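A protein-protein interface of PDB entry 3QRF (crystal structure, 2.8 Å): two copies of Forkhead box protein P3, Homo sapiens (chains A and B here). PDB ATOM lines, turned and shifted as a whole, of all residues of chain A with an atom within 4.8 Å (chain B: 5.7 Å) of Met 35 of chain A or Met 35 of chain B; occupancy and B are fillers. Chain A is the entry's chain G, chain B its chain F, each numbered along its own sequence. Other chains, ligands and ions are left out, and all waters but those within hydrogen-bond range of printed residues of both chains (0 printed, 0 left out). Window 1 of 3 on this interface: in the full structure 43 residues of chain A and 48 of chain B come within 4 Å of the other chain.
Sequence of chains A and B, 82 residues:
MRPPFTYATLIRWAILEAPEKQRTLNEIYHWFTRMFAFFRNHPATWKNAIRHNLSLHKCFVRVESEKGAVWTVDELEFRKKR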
ATOM      1  N   PHE A   5     -14.012  18.770 -18.456  1.00  0.00           N
ATOM      2  CA  PHE A   5     -13.460  18.784 -19.779  1.00  0.00           C
ATOM      3  C   PHE A   5     -14.468  19.613 -20.594  1.00  0.00           C
ATOM      4  O   PHE A   5     -15.690  19.409 -20.509  1.00  0.00           O
ATOM      5  CB  PHE A   5     -13.426  17.370 -20.327  1.00  0.00           C
ATOM      6  CG  PHE A   5     -12.716  16.400 -19.454  1.00  0.00           C
ATOM      7  CD1 PHE A   5     -13.350  15.232 -19.043  1.00  0.00           C
ATOM      8  CD2 PHE A   5     -11.395  16.613 -19.093  1.00  0.00           C
ATOM      9  CE1 PHE A   5     -12.676  14.288 -18.290  1.00  0.00           C
ATOM     10  CE2 PHE A   5     -10.709  15.679 -18.340  1.00  0.00           C
ATOM     11  CZ  PHE A   5     -11.350  14.512 -17.938  1.00  0.00           C
ATOM     12  N   LEU A  10     -14.587  16.756 -25.058  1.00  0.00           N
ATOM     13  CA  LEU A  10     -15.521  15.652 -25.087  1.00  0.00           C
ATOM     14  C   LEU A  10     -15.918  15.290 -26.523  1.00  0.00           C
ATOM     15  O   LEU A  10     -15.832  14.127 -26.923  1.00  0.00           O
ATOM     16  CB  LEU A  10     -16.740  15.998 -24.240  1.00  0.00           C
ATOM     17  CG  LEU A  10     -16.393  16.220 -22.766  1.00  0.00           C
ATOM     18  CD1 LEU A  10     -17.484  16.994 -22.034  1.00  0.00           C
ATOM     19  CD2 LEU A  10     -16.196  14.895 -22.121  1.00  0.00           C
ATOM     20  N   TRP A  13     -13.254  13.310 -28.199  1.00  0.00           N
ATOM     21  CA  TRP A  13     -13.211  11.930 -27.768  1.00  0.00           C
ATOM     22  C   TRP A  13     -14.319  11.130 -28.431  1.00  0.00           C
ATOM     23  O   TRP A  13     -14.099  10.009 -28.873  1.00  0.00           O
ATOM     24  CB  TRP A  13     -13.349  11.802 -26.254  1.00  0.00           C
ATOM     25  CG  TRP A  13     -12.141  12.155 -25.488  1.00  0.00           C
ATOM     26  CD1 TRP A  13     -10.863  12.145 -25.934  1.00  0.00           C
ATOM     27  CD2 TRP A  13     -12.093  12.618 -24.134  1.00  0.00           C
ATOM     28  NE1 TRP A  13     -10.004  12.589 -24.946  1.00  0.00           N
ATOM     29  CE2 TRP A  13     -10.735  12.884 -23.830  1.00  0.00           C
ATOM     30  CE3 TRP A  13     -13.065  12.835 -23.148  1.00  0.00           C
ATOM     31  CZ2 TRP A  13     -10.321  13.360 -22.585  1.00  0.00           C
ATOM     32  CZ3 TRP A  13     -12.655  13.309 -21.905  1.00  0.00           C
ATOM     33  CH2 TRP A  13     -11.289  13.568 -21.635  1.00  0.00           C
ATOM     34  N   TRP A  31     -22.876   9.108 -27.965  1.00  0.00           N
ATOM     35  CA  TRP A  31     -21.662   8.903 -27.192  1.00  0.00           C
ATOM     36  C   TRP A  31     -21.885   9.654 -25.892  1.00  0.00           C
ATOM     37  O   TRP A  31     -21.597   9.140 -24.831  1.00  0.00           O
ATOM     38  CB  TRP A  31     -20.450   9.475 -27.908  1.00  0.00           C
ATOM     39  CG  TRP A  31     -19.209   9.311 -27.127  1.00  0.00           C
ATOM     40  CD1 TRP A  31     -18.308   8.292 -27.220  1.00  0.00           C
ATOM     41  CD2 TRP A  31     -18.697  10.213 -26.142  1.00  0.00           C
ATOM     42  NE1 TRP A  31     -17.257   8.510 -26.360  1.00  0.00           N
ATOM     43  CE2 TRP A  31     -17.473   9.684 -25.688  1.00  0.00           C
ATOM     44  CE3 TRP A  31     -19.156  11.424 -25.602  1.00  0.00           C
ATOM     45  CZ2 TRP A  31     -16.703  10.320 -24.727  1.00  0.00           C
ATOM     46  CZ3 TRP A  31     -18.393  12.053 -24.646  1.00  0.00           C
ATOM     47  CH2 TRP A  31     -17.177  11.502 -24.217  1.00  0.00           C
ATOM     48  N   PHE A  32     -22.405  10.873 -25.982  1.00  0.00           N
ATOM     49  CA  PHE A  32     -22.692  11.658 -24.788  1.00  0.00           C
ATOM     50  C   PHE A  32     -23.754  10.986 -23.907  1.00  0.00           C
ATOM     51  O   PHE A  32     -23.638  10.964 -22.678  1.00  0.00           O
ATOM     52  CB  PHE A  32     -23.201  13.047 -25.157  1.00  0.00           C
ATOM     53  CG  PHE A  32     -22.128  14.076 -25.251  1.00  0.00           C
ATOM     54  CD1 PHE A  32     -21.221  14.064 -26.309  1.00  0.00           C
ATOM     55  CD2 PHE A  32     -22.002  15.053 -24.264  1.00  0.00           C
ATOM     56  CE1 PHE A  32     -20.206  15.004 -26.375  1.00  0.00           C
ATOM     57  CE2 PHE A  32     -20.991  15.989 -24.328  1.00  0.00           C
ATOM     58  CZ  PHE A  32     -20.087  15.962 -25.391  1.00  0.00           C
ATOM     59  N   THR A  33     -24.798  10.457 -24.532  1.00  0.00           N
ATOM     60  CA  THR A  33     -25.850   9.826 -23.774  1.00  0.00           C
ATOM     61  C   THR A  33     -25.299   8.639 -23.002  1.00  0.00           C
ATOM     62  O   THR A  33     -25.594   8.481 -21.816  1.00  0.00           O
ATOM     63  CB  THR A  33     -27.019   9.405 -24.704  1.00  0.00           C
ATOM     64  OG1 THR A  33     -27.810  10.562 -25.003  1.00  0.00           O
ATOM     65  CG2 THR A  33     -27.908   8.368 -24.042  1.00  0.00           C
ATOM     66  N   ARG A  34     -24.489   7.814 -23.660  1.00  0.00           N
ATOM     67  CA  ARG A  34     -23.901   6.663 -22.985  1.00  0.00           C
ATOM     68  C   ARG A  34     -23.075   7.126 -21.795  1.00  0.00           C
ATOM     69  O   ARG A  34     -23.065   6.486 -20.750  1.00  0.00           O
ATOM     70  CB  ARG A  34     -23.025   5.855 -23.942  1.00  0.00           C
ATOM     71  CG  ARG A  34     -23.799   4.954 -24.883  1.00  0.00           C
ATOM     72  CD  ARG A  34     -23.226   5.038 -26.301  1.00  0.00           C
ATOM     73  NE  ARG A  34     -21.880   4.478 -26.426  1.00  0.00           N
ATOM     74  CZ  ARG A  34     -21.066   4.718 -27.454  1.00  0.00           C
ATOM     75  NH1 ARG A  34     -21.469   5.517 -28.443  1.00  0.00           N
ATOM     76  NH2 ARG A  34     -19.856   4.162 -27.503  1.00  0.00           N
ATOM     77  N   MET A  35     -22.402   8.256 -21.941  1.00  0.00           N
ATOM     78  CA  MET A  35     -21.593   8.752 -20.849  1.00  0.00           C
ATOM     79  C   MET A  35     -22.487   9.231 -19.715  1.00  0.00           C
ATOM     80  O   MET A  35     -22.132   9.098 -18.552  1.00  0.00           O
ATOM     81  CB  MET A  35     -20.686   9.884 -21.326  1.00  0.00           C
ATOM     82  CG  MET A  35     -19.392  10.043 -20.518  1.00  0.00           C
ATOM     83  SD  MET A  35     -18.263   8.579 -20.500  1.00  0.00           S
ATOM     84  CE  MET A  35     -17.158   8.941 -21.810  1.00  0.00           C
ATOM     85  N   PHE A  36     -23.644   9.799 -20.037  1.00  0.00           N
ATOM     86  CA  PHE A  36     -24.552  10.272 -18.988  1.00  0.00           C
ATOM     87  C   PHE A  36     -25.049   9.032 -18.264  1.00  0.00           C
ATOM     88  O   PHE A  36     -25.115   8.992 -17.032  1.00  0.00           O
ATOM     89  CB  PHE A  36     -25.768  10.992 -19.576  1.00  0.00           C
ATOM     90  CG  PHE A  36     -25.488  12.376 -20.089  1.00  0.00           C
ATOM     91  CD1 PHE A  36     -25.966  12.772 -21.348  1.00  0.00           C
ATOM     92  CD2 PHE A  36     -24.805  13.297 -19.312  1.00  0.00           C
ATOM     93  CE1 PHE A  36     -25.764  14.068 -21.820  1.00  0.00           C
ATOM     94  CE2 PHE A  36     -24.595  14.600 -19.774  1.00  0.00           C
ATOM     95  CZ  PHE A  36     -25.076  14.988 -21.032  1.00  0.00           C
ATOM     96  N   ALA A  37     -25.407   8.024 -19.054  1.00  0.00           N
ATOM     97  CA  ALA A  37     -25.906   6.775 -18.521  1.00  0.00           C
ATOM     98  C   ALA A  37     -24.937   6.266 -17.483  1.00  0.00           C
ATOM     99  O   ALA A  37     -25.321   5.953 -16.361  1.00  0.00           O
ATOM    100  CB  ALA A  37     -26.045   5.762 -19.624  1.00  0.00           C
ATOM    101  N   PHE A  38     -23.667   6.199 -17.850  1.00  0.00           N
ATOM    102  CA  PHE A  38     -22.664   5.706 -16.934  1.00  0.00           C
ATOM    103  C   PHE A  38     -22.582   6.459 -15.627  1.00  0.00           C
ATOM    104  O   PHE A  38     -22.998   5.958 -14.597  1.00  0.00           O
ATOM    105  CB  PHE A  38     -21.280   5.723 -17.571  1.00  0.00           C
ATOM    106  CG  PHE A  38     -20.235   5.065 -16.727  1.00  0.00           C
ATOM    107  CD1 PHE A  38     -20.054   3.687 -16.779  1.00  0.00           C
ATOM    108  CD2 PHE A  38     -19.487   5.809 -15.820  1.00  0.00           C
ATOM    109  CE1 PHE A  38     -19.140   3.057 -15.921  1.00  0.00           C
ATOM    110  CE2 PHE A  38     -18.579   5.199 -14.966  1.00  0.00           C
ATOM    111  CZ  PHE A  38     -18.401   3.820 -15.009  1.00  0.00           C
ATOM    112  N   PHE A  39     -22.048   7.667 -15.660  1.00  0.00           N
ATOM    113  CA  PHE A  39     -21.868   8.419 -14.430  1.00  0.00           C
ATOM    114  C   PHE A  39     -23.092   8.636 -13.569  1.00  0.00           C
ATOM    115  O   PHE A  39     -22.981   9.039 -12.413  1.00  0.00           O
ATOM    116  CB  PHE A  39     -21.184   9.732 -14.750  1.00  0.00           C
ATOM    117  CG  PHE A  39     -19.815   9.544 -15.328  1.00  0.00           C
ATOM    118  CD1 PHE A  39     -19.658   9.063 -16.625  1.00  0.00           C
ATOM    119  CD2 PHE A  39     -18.686   9.768 -14.556  1.00  0.00           C
ATOM    120  CE1 PHE A  39     -18.410   8.808 -17.140  1.00  0.00           C
ATOM    121  CE2 PHE A  39     -17.438   9.517 -15.062  1.00  0.00           C
ATOM    122  CZ  PHE A  39     -17.299   9.031 -16.363  1.00  0.00           C
ATOM    123  N   PHE B   5     -21.034   1.955 -21.590  1.00  0.00           N
ATOM    124  CA  PHE B   5     -19.682   2.121 -21.092  1.00  0.00           C
ATOM    125  C   PHE B   5     -19.395   1.241 -19.891  1.00  0.00           C
ATOM    126  O   PHE B   5     -20.205   1.124 -18.971  1.00  0.00           O
ATOM    127  CB  PHE B   5     -19.428   3.576 -20.730  1.00  0.00           C
ATOM    128  CG  PHE B   5     -19.326   4.479 -21.918  1.00  0.00           C
ATOM    129  CD1 PHE B   5     -19.373   5.863 -21.760  1.00  0.00           C
ATOM    130  CD2 PHE B   5     -19.174   3.950 -23.196  1.00  0.00           C
ATOM    131  CE1 PHE B   5     -19.274   6.700 -22.838  1.00  0.00           C
ATOM    132  CE2 PHE B   5     -19.071   4.784 -24.292  1.00  0.00           C
ATOM    133  CZ  PHE B   5     -19.122   6.166 -24.114  1.00  0.00           C
ATOM    134  N   LEU B  10     -13.741   2.843 -20.025  1.00  0.00           N
ATOM    135  CA  LEU B  10     -13.375   4.181 -19.602  1.00  0.00           C
ATOM    136  C   LEU B  10     -11.923   4.186 -19.110  1.00  0.00           C
ATOM    137  O   LEU B  10     -11.134   5.040 -19.465  1.00  0.00           O
ATOM    138  CB  LEU B  10     -14.322   4.667 -18.505  1.00  0.00           C
ATOM    139  CG  LEU B  10     -15.715   5.004 -19.052  1.00  0.00           C
ATOM    140  CD1 LEU B  10     -16.727   5.129 -17.934  1.00  0.00           C
ATOM    141  CD2 LEU B  10     -15.633   6.296 -19.848  1.00  0.00           C
ATOM    142  N   HIS B  30      -8.661  11.332 -11.043  1.00  0.00           N
ATOM    143  CA  HIS B  30      -8.872  12.696 -11.513  1.00  0.00           C
ATOM    144  C   HIS B  30      -9.660  12.768 -12.793  1.00  0.00           C
ATOM    145  O   HIS B  30     -10.619  13.540 -12.910  1.00  0.00           O
ATOM    146  CB  HIS B  30      -7.547  13.418 -11.704  1.00  0.00           C
ATOM    147  CG  HIS B  30      -7.035  14.050 -10.451  1.00  0.00           C
ATOM    148  ND1 HIS B  30      -6.607  13.313  -9.365  1.00  0.00           N
ATOM    149  CD2 HIS B  30      -6.910  15.351 -10.098  1.00  0.00           C
ATOM    150  CE1 HIS B  30      -6.239  14.135  -8.397  1.00  0.00           C
ATOM    151  NE2 HIS B  30      -6.413  15.377  -8.816  1.00  0.00           N
ATOM    152  N   TRP B  31      -9.248  11.960 -13.756  1.00  0.00           N
ATOM    153  CA  TRP B  31      -9.924  11.925 -15.031  1.00  0.00           C
ATOM    154  C   TRP B  31     -11.404  11.657 -14.795  1.00  0.00           C
ATOM    155  O   TRP B  31     -12.243  12.436 -15.222  1.00  0.00           O
ATOM    156  CB  TRP B  31      -9.323  10.829 -15.898  1.00  0.00           C
ATOM    157  CG  TRP B  31      -9.778  10.871 -17.295  1.00  0.00           C
ATOM    158  CD1 TRP B  31      -9.315  11.679 -18.277  1.00  0.00           C
ATOM    159  CD2 TRP B  31     -10.806  10.073 -17.874  1.00  0.00           C
ATOM    160  NE1 TRP B  31      -9.991  11.432 -19.448  1.00  0.00           N
ATOM    161  CE2 TRP B  31     -10.914  10.448 -19.225  1.00  0.00           C
ATOM    162  CE3 TRP B  31     -11.647   9.075 -17.381  1.00  0.00           C
ATOM    163  CZ2 TRP B  31     -11.828   9.861 -20.092  1.00  0.00           C
ATOM    164  CZ3 TRP B  31     -12.554   8.489 -18.243  1.00  0.00           C
ATOM    165  CH2 TRP B  31     -12.637   8.884 -19.583  1.00  0.00           C
ATOM    166  N   PHE B  32     -11.731  10.573 -14.095  1.00  0.00           N
ATOM    167  CA  PHE B  32     -13.134  10.246 -13.837  1.00  0.00           C
ATOM    168  C   PHE B  32     -13.923  11.396 -13.214  1.00  0.00           C
ATOM    169  O   PHE B  32     -15.086  11.642 -13.549  1.00  0.00           O
ATOM    170  CB  PHE B  32     -13.240   9.004 -12.944  1.00  0.00           C
ATOM    171  CG  PHE B  32     -13.256   7.712 -13.715  1.00  0.00           C
ATOM    172  CD1 PHE B  32     -12.094   7.216 -14.295  1.00  0.00           C
ATOM    173  CD2 PHE B  32     -14.440   7.003 -13.879  1.00  0.00           C
ATOM    174  CE1 PHE B  32     -12.104   6.029 -15.032  1.00  0.00           C
ATOM    175  CE2 PHE B  32     -14.467   5.828 -14.603  1.00  0.00           C
ATOM    176  CZ  PHE B  32     -13.288   5.336 -15.187  1.00  0.00           C
ATOM    177  N   THR B  33     -13.270  12.098 -12.306  1.00  0.00           N
ATOM    178  CA  THR B  33     -13.863  13.217 -11.614  1.00  0.00           C
ATOM    179  C   THR B  33     -14.308  14.308 -12.591  1.00  0.00           C
ATOM    180  O   THR B  33     -15.452  14.756 -12.564  1.00  0.00           O
ATOM    181  CB  THR B  33     -12.843  13.796 -10.617  1.00  0.00           C
ATOM    182  OG1 THR B  33     -12.497  12.782  -9.659  1.00  0.00           O
ATOM    183  CG2 THR B  33     -13.421  15.009  -9.899  1.00  0.00           C
ATOM    184  N   ARG B  34     -13.398  14.743 -13.452  1.00  0.00           N
ATOM    185  CA  ARG B  34     -13.736  15.784 -14.408  1.00  0.00           C
ATOM    186  C   ARG B  34     -14.889  15.317 -15.276  1.00  0.00           C
ATOM    187  O   ARG B  34     -15.670  16.117 -15.778  1.00  0.00           O
ATOM    188  CB  ARG B  34     -12.527  16.135 -15.274  1.00  0.00           C
ATOM    189  CG  ARG B  34     -11.295  16.571 -14.468  1.00  0.00           C
ATOM    190  CD  ARG B  34     -10.257  17.238 -15.366  1.00  0.00           C
ATOM    191  NE  ARG B  34     -10.881  18.338 -16.098  1.00  0.00           N
ATOM    192  CZ  ARG B  34     -10.355  18.943 -17.153  1.00  0.00           C
ATOM    193  NH1 ARG B  34      -9.172  18.563 -17.618  1.00  0.00           N
ATOM    194  NH2 ARG B  34     -11.037  19.910 -17.759  1.00  0.00           N
ATOM    195  N   MET B  35     -15.006  14.011 -15.450  1.00  0.00           N
ATOM    196  CA  MET B  35     -16.093  13.498 -16.251  1.00  0.00           C
ATOM    197  C   MET B  35     -17.372  13.590 -15.418  1.00  0.00           C
ATOM    198  O   MET B  35     -18.421  13.962 -15.944  1.00  0.00           O
ATOM    199  CB  MET B  35     -15.820  12.064 -16.664  1.00  0.00           C
ATOM    200  CG  MET B  35     -16.518  11.677 -17.938  1.00  0.00           C
ATOM    201  SD  MET B  35     -15.627  12.211 -19.401  1.00  0.00           S
ATOM    202  CE  MET B  35     -15.175  10.619 -20.046  1.00  0.00           C
ATOM    203  N   PHE B  36     -17.284  13.252 -14.126  1.00  0.00           N
ATOM    204  CA  PHE B  36     -18.437  13.349 -13.213  1.00  0.00           C
ATOM    205  C   PHE B  36     -18.841  14.813 -13.175  1.00  0.00           C
ATOM    206  O   PHE B  36     -20.013  15.152 -13.260  1.00  0.00           O
ATOM    207  CB  PHE B  36     -18.077  12.972 -11.758  1.00  0.00           C
ATOM    208  CG  PHE B  36     -18.322  11.533 -11.402  1.00  0.00           C
ATOM    209  CD1 PHE B  36     -19.542  10.921 -11.688  1.00  0.00           C
ATOM    210  CD2 PHE B  36     -17.330  10.788 -10.759  1.00  0.00           C
ATOM    211  CE1 PHE B  36     -19.772   9.570 -11.339  1.00  0.00           C
ATOM    212  CE2 PHE B  36     -17.544   9.444 -10.405  1.00  0.00           C
ATOM    213  CZ  PHE B  36     -18.767   8.832 -10.695  1.00  0.00           C
ATOM    214  N   ALA B  37     -17.840  15.676 -13.035  1.00  0.00           N
ATOM    215  CA  ALA B  37     -18.061  17.105 -12.946  1.00  0.00           C
ATOM    216  C   ALA B  37     -18.574  17.735 -14.223  1.00  0.00           C
ATOM    217  O   ALA B  37     -18.478  18.941 -14.392  1.00  0.00           O
ATOM    218  CB  ALA B  37     -16.791  17.794 -12.509  1.00  0.00           C
ATOM    219  N   PHE B  38     -19.095  16.924 -15.132  1.00  0.00           N
ATOM    220  CA  PHE B  38     -19.649  17.432 -16.369  1.00  0.00           C
ATOM    221  C   PHE B  38     -20.972  16.740 -16.527  1.00  0.00           C
ATOM    222  O   PHE B  38     -21.995  17.382 -16.686  1.00  0.00           O
ATOM    223  CB  PHE B  38     -18.782  17.086 -17.578  1.00  0.00           C
ATOM    224  CG  PHE B  38     -19.445  17.393 -18.906  1.00  0.00           C
ATOM    225  CD1 PHE B  38     -19.347  18.651 -19.474  1.00  0.00           C
ATOM    226  CD2 PHE B  38     -20.218  16.428 -19.556  1.00  0.00           C
ATOM    227  CE1 PHE B  38     -20.010  18.946 -20.663  1.00  0.00           C
ATOM    228  CE2 PHE B  38     -20.891  16.713 -20.754  1.00  0.00           C
ATOM    229  CZ  PHE B  38     -20.786  17.972 -21.304  1.00  0.00           C
ATOM    230  N   PHE B  39     -20.940  15.416 -16.482  1.00  0.00           N
ATOM    231  CA  PHE B  39     -22.141  14.619 -16.645  1.00  0.00           C
ATOM    232  C   PHE B  39     -23.017  14.574 -15.400  1.00  0.00           C
ATOM    233  O   PHE B  39     -23.435  13.498 -14.958  1.00  0.00           O
ATOM    234  CB  PHE B  39     -21.756  13.214 -17.085  1.00  0.00           C
ATOM    235  CG  PHE B  39     -20.992  13.185 -18.387  1.00  0.00           C
ATOM    236  CD1 PHE B  39     -19.607  13.054 -18.400  1.00  0.00           C
ATOM    237  CD2 PHE B  39     -21.659  13.314 -19.602  1.00  0.00           C
ATOM    238  CE1 PHE B  39     -18.905  13.053 -19.601  1.00  0.00           C
ATOM    239  CE2 PHE B  39     -20.965  13.311 -20.799  1.00  0.00           C
ATOM    240  CZ  PHE B  39     -19.583  13.182 -20.798  1.00  0.00           C
ATOM    241  N   ARG B  40     -23.284  15.764 -14.857  1.00  0.00           N
ATOM    242  CA  ARG B  40     -24.115  15.965 -13.667  1.00  0.00           C
ATOM    243  C   ARG B  40     -24.404  17.473 -13.602  1.00  0.00           C
ATOM    244  O   ARG B  40     -25.145  17.962 -12.728  1.00  0.00           O
ATOM    245  CB  ARG B  40     -23.360  15.546 -12.401  1.00  0.00           C
ATOM    246  CG  ARG B  40     -22.273  16.535 -12.009  1.00  0.00           C
ATOM    247  CD  ARG B  40     -21.579  16.174 -10.703  1.00  0.00           C
ATOM    248  NE  ARG B  40     -20.504  17.124 -10.418  1.00  0.00           N
ATOM    249  CZ  ARG B  40     -19.700  17.069  -9.361  1.00  0.00           C
ATOM    250  NH1 ARG B  40     -19.839  16.097  -8.465  1.00  0.00           N
ATOM    251  NH2 ARG B  40     -18.760  17.996  -9.201  1.00  0.00           N
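The guanidinium group (NH2) of Arg 34 of chain B sits close to the backbone NH (N) of Phe 5 of chain A, at 3.3 Å.
The guanidinium group (NE) of Arg 40 of chain B lies close to the backbone carbonyl oxygen (O) of Phe 36 of chain B, 3.5 Å away.
Among the printed residues, pairs that only touch across the chains: Met 35 of chain A with Met 35 of chain B (3.1 Å), Met 35 of chain A with Phe 39 of chain B (3.2 Å), Phe 36 of chain A with Phe 39 of chain B (3.2 Å), Met 35 of chain A with Phe 5 of chain B (3.2 Å), Phe 39 of chain A with Met 35 of chain B (3.2 Å), Phe 39 of chain A with Phe 36 of chain B (3.2 Å), Trp 13 of chain A with Trp 31 of chain B (3.3 Å), Arg 34 of chain A with Phe 5 of chain B (3.4 Å), Phe 38 of chain A with Phe 5 of chain B (3.4 Å), Leu 10 of chain A with Phe 38 of chain B (3.5 Å), Phe 38 of chain A with Leu 10 of chain B (3.5 Å), Phe 5 of chain A with Trp 31 of chain B (3.5 Å), Phe 39 of chain A with Phe 32 of chain B (3.5 Å), Met 35 of chain A with Leu 10 of chain B (3.5 Å), Phe 32 of chain A with Phe 38 of chain B (3.6 Å), Phe 5 of chain A with Met 35 of chain B (3.7 Å), Trp 31 of chain A with Phe 5 of chain B (3.7 Å), Leu 10 of chain A with Met 35 of chain B (3.9 Å) and Phe 5 of chain A with Phe 38 of chain B (3.9 Å).
Printed residues of chain B within 4 Å of Phe 38 of chain A: Phe 5 and Leu 10.
Of the printed residues of chain A, Leu 10 of chain B touches Met 35 and Phe 38.
Met 35 of chain B touches just these residues of chain A: Phe 5 (3.7 Å), Leu 10 (3.9 Å), Met 35 (3.1 Å) and Phe 39 (3.2 Å).
The nearest residue of chain B that does not touch Met 35 of chain A is Trp 31 of chain B (5.0 Å).
The nearest printed residue of chain B that does not touch Leu 10 of chain A is Phe 39 of chain B (4.02 Å).
Printed residues of chain A that touch a printed residue of chain B: Phe 5, Leu 10, Trp 13, Trp 31, Phe 32, Arg 34, Met 35, Phe 36, Phe 38 and Phe 39.
Hydrophobic or aromatic side chains of chain A within 4 Å of the printed part of chain B: Phe 5, Leu 10, Trp 13, Trp 31, Phe 32, Met 35, Phe 36, Phe 38 and Phe 39.
Of the 13 printed residues of chain B, 9 touch a printed residue of chain A.
Printed residues of chain B that touch a printed residue of chain A: Phe 5, Leu 10, Trp 31, Phe 32, Arg 34, Met 35, Phe 36, Phe 38 and Phe 39.
Hydrophobic or aromatic side chains of chain B within 4 Å of the printed part of chain A: Phe 5, Leu 10, Trp 31, Met 35, Phe 36, Phe 38 and Phe 39.
Phe 5 of chain A touches Trp 31 of chain B, and with the chains exchanged Trp 31 of chain A touches Phe 5 of chain B.
Phe 5 of chain A touches Arg 34 of chain B, and with the chains exchanged Arg 34 of chain A touches Phe 5 of chain B.
Phe 5 of chain A touches Met 35 of chain B, and with the chains exchanged Met 35 of chain A touches Phe 5 of chain B.
Phe 39 of chain A touches Phe 32 of chain B, but with the chains exchanged Phe 32 of chain A does not touch Phe 39 of chain B (4.01 Å).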
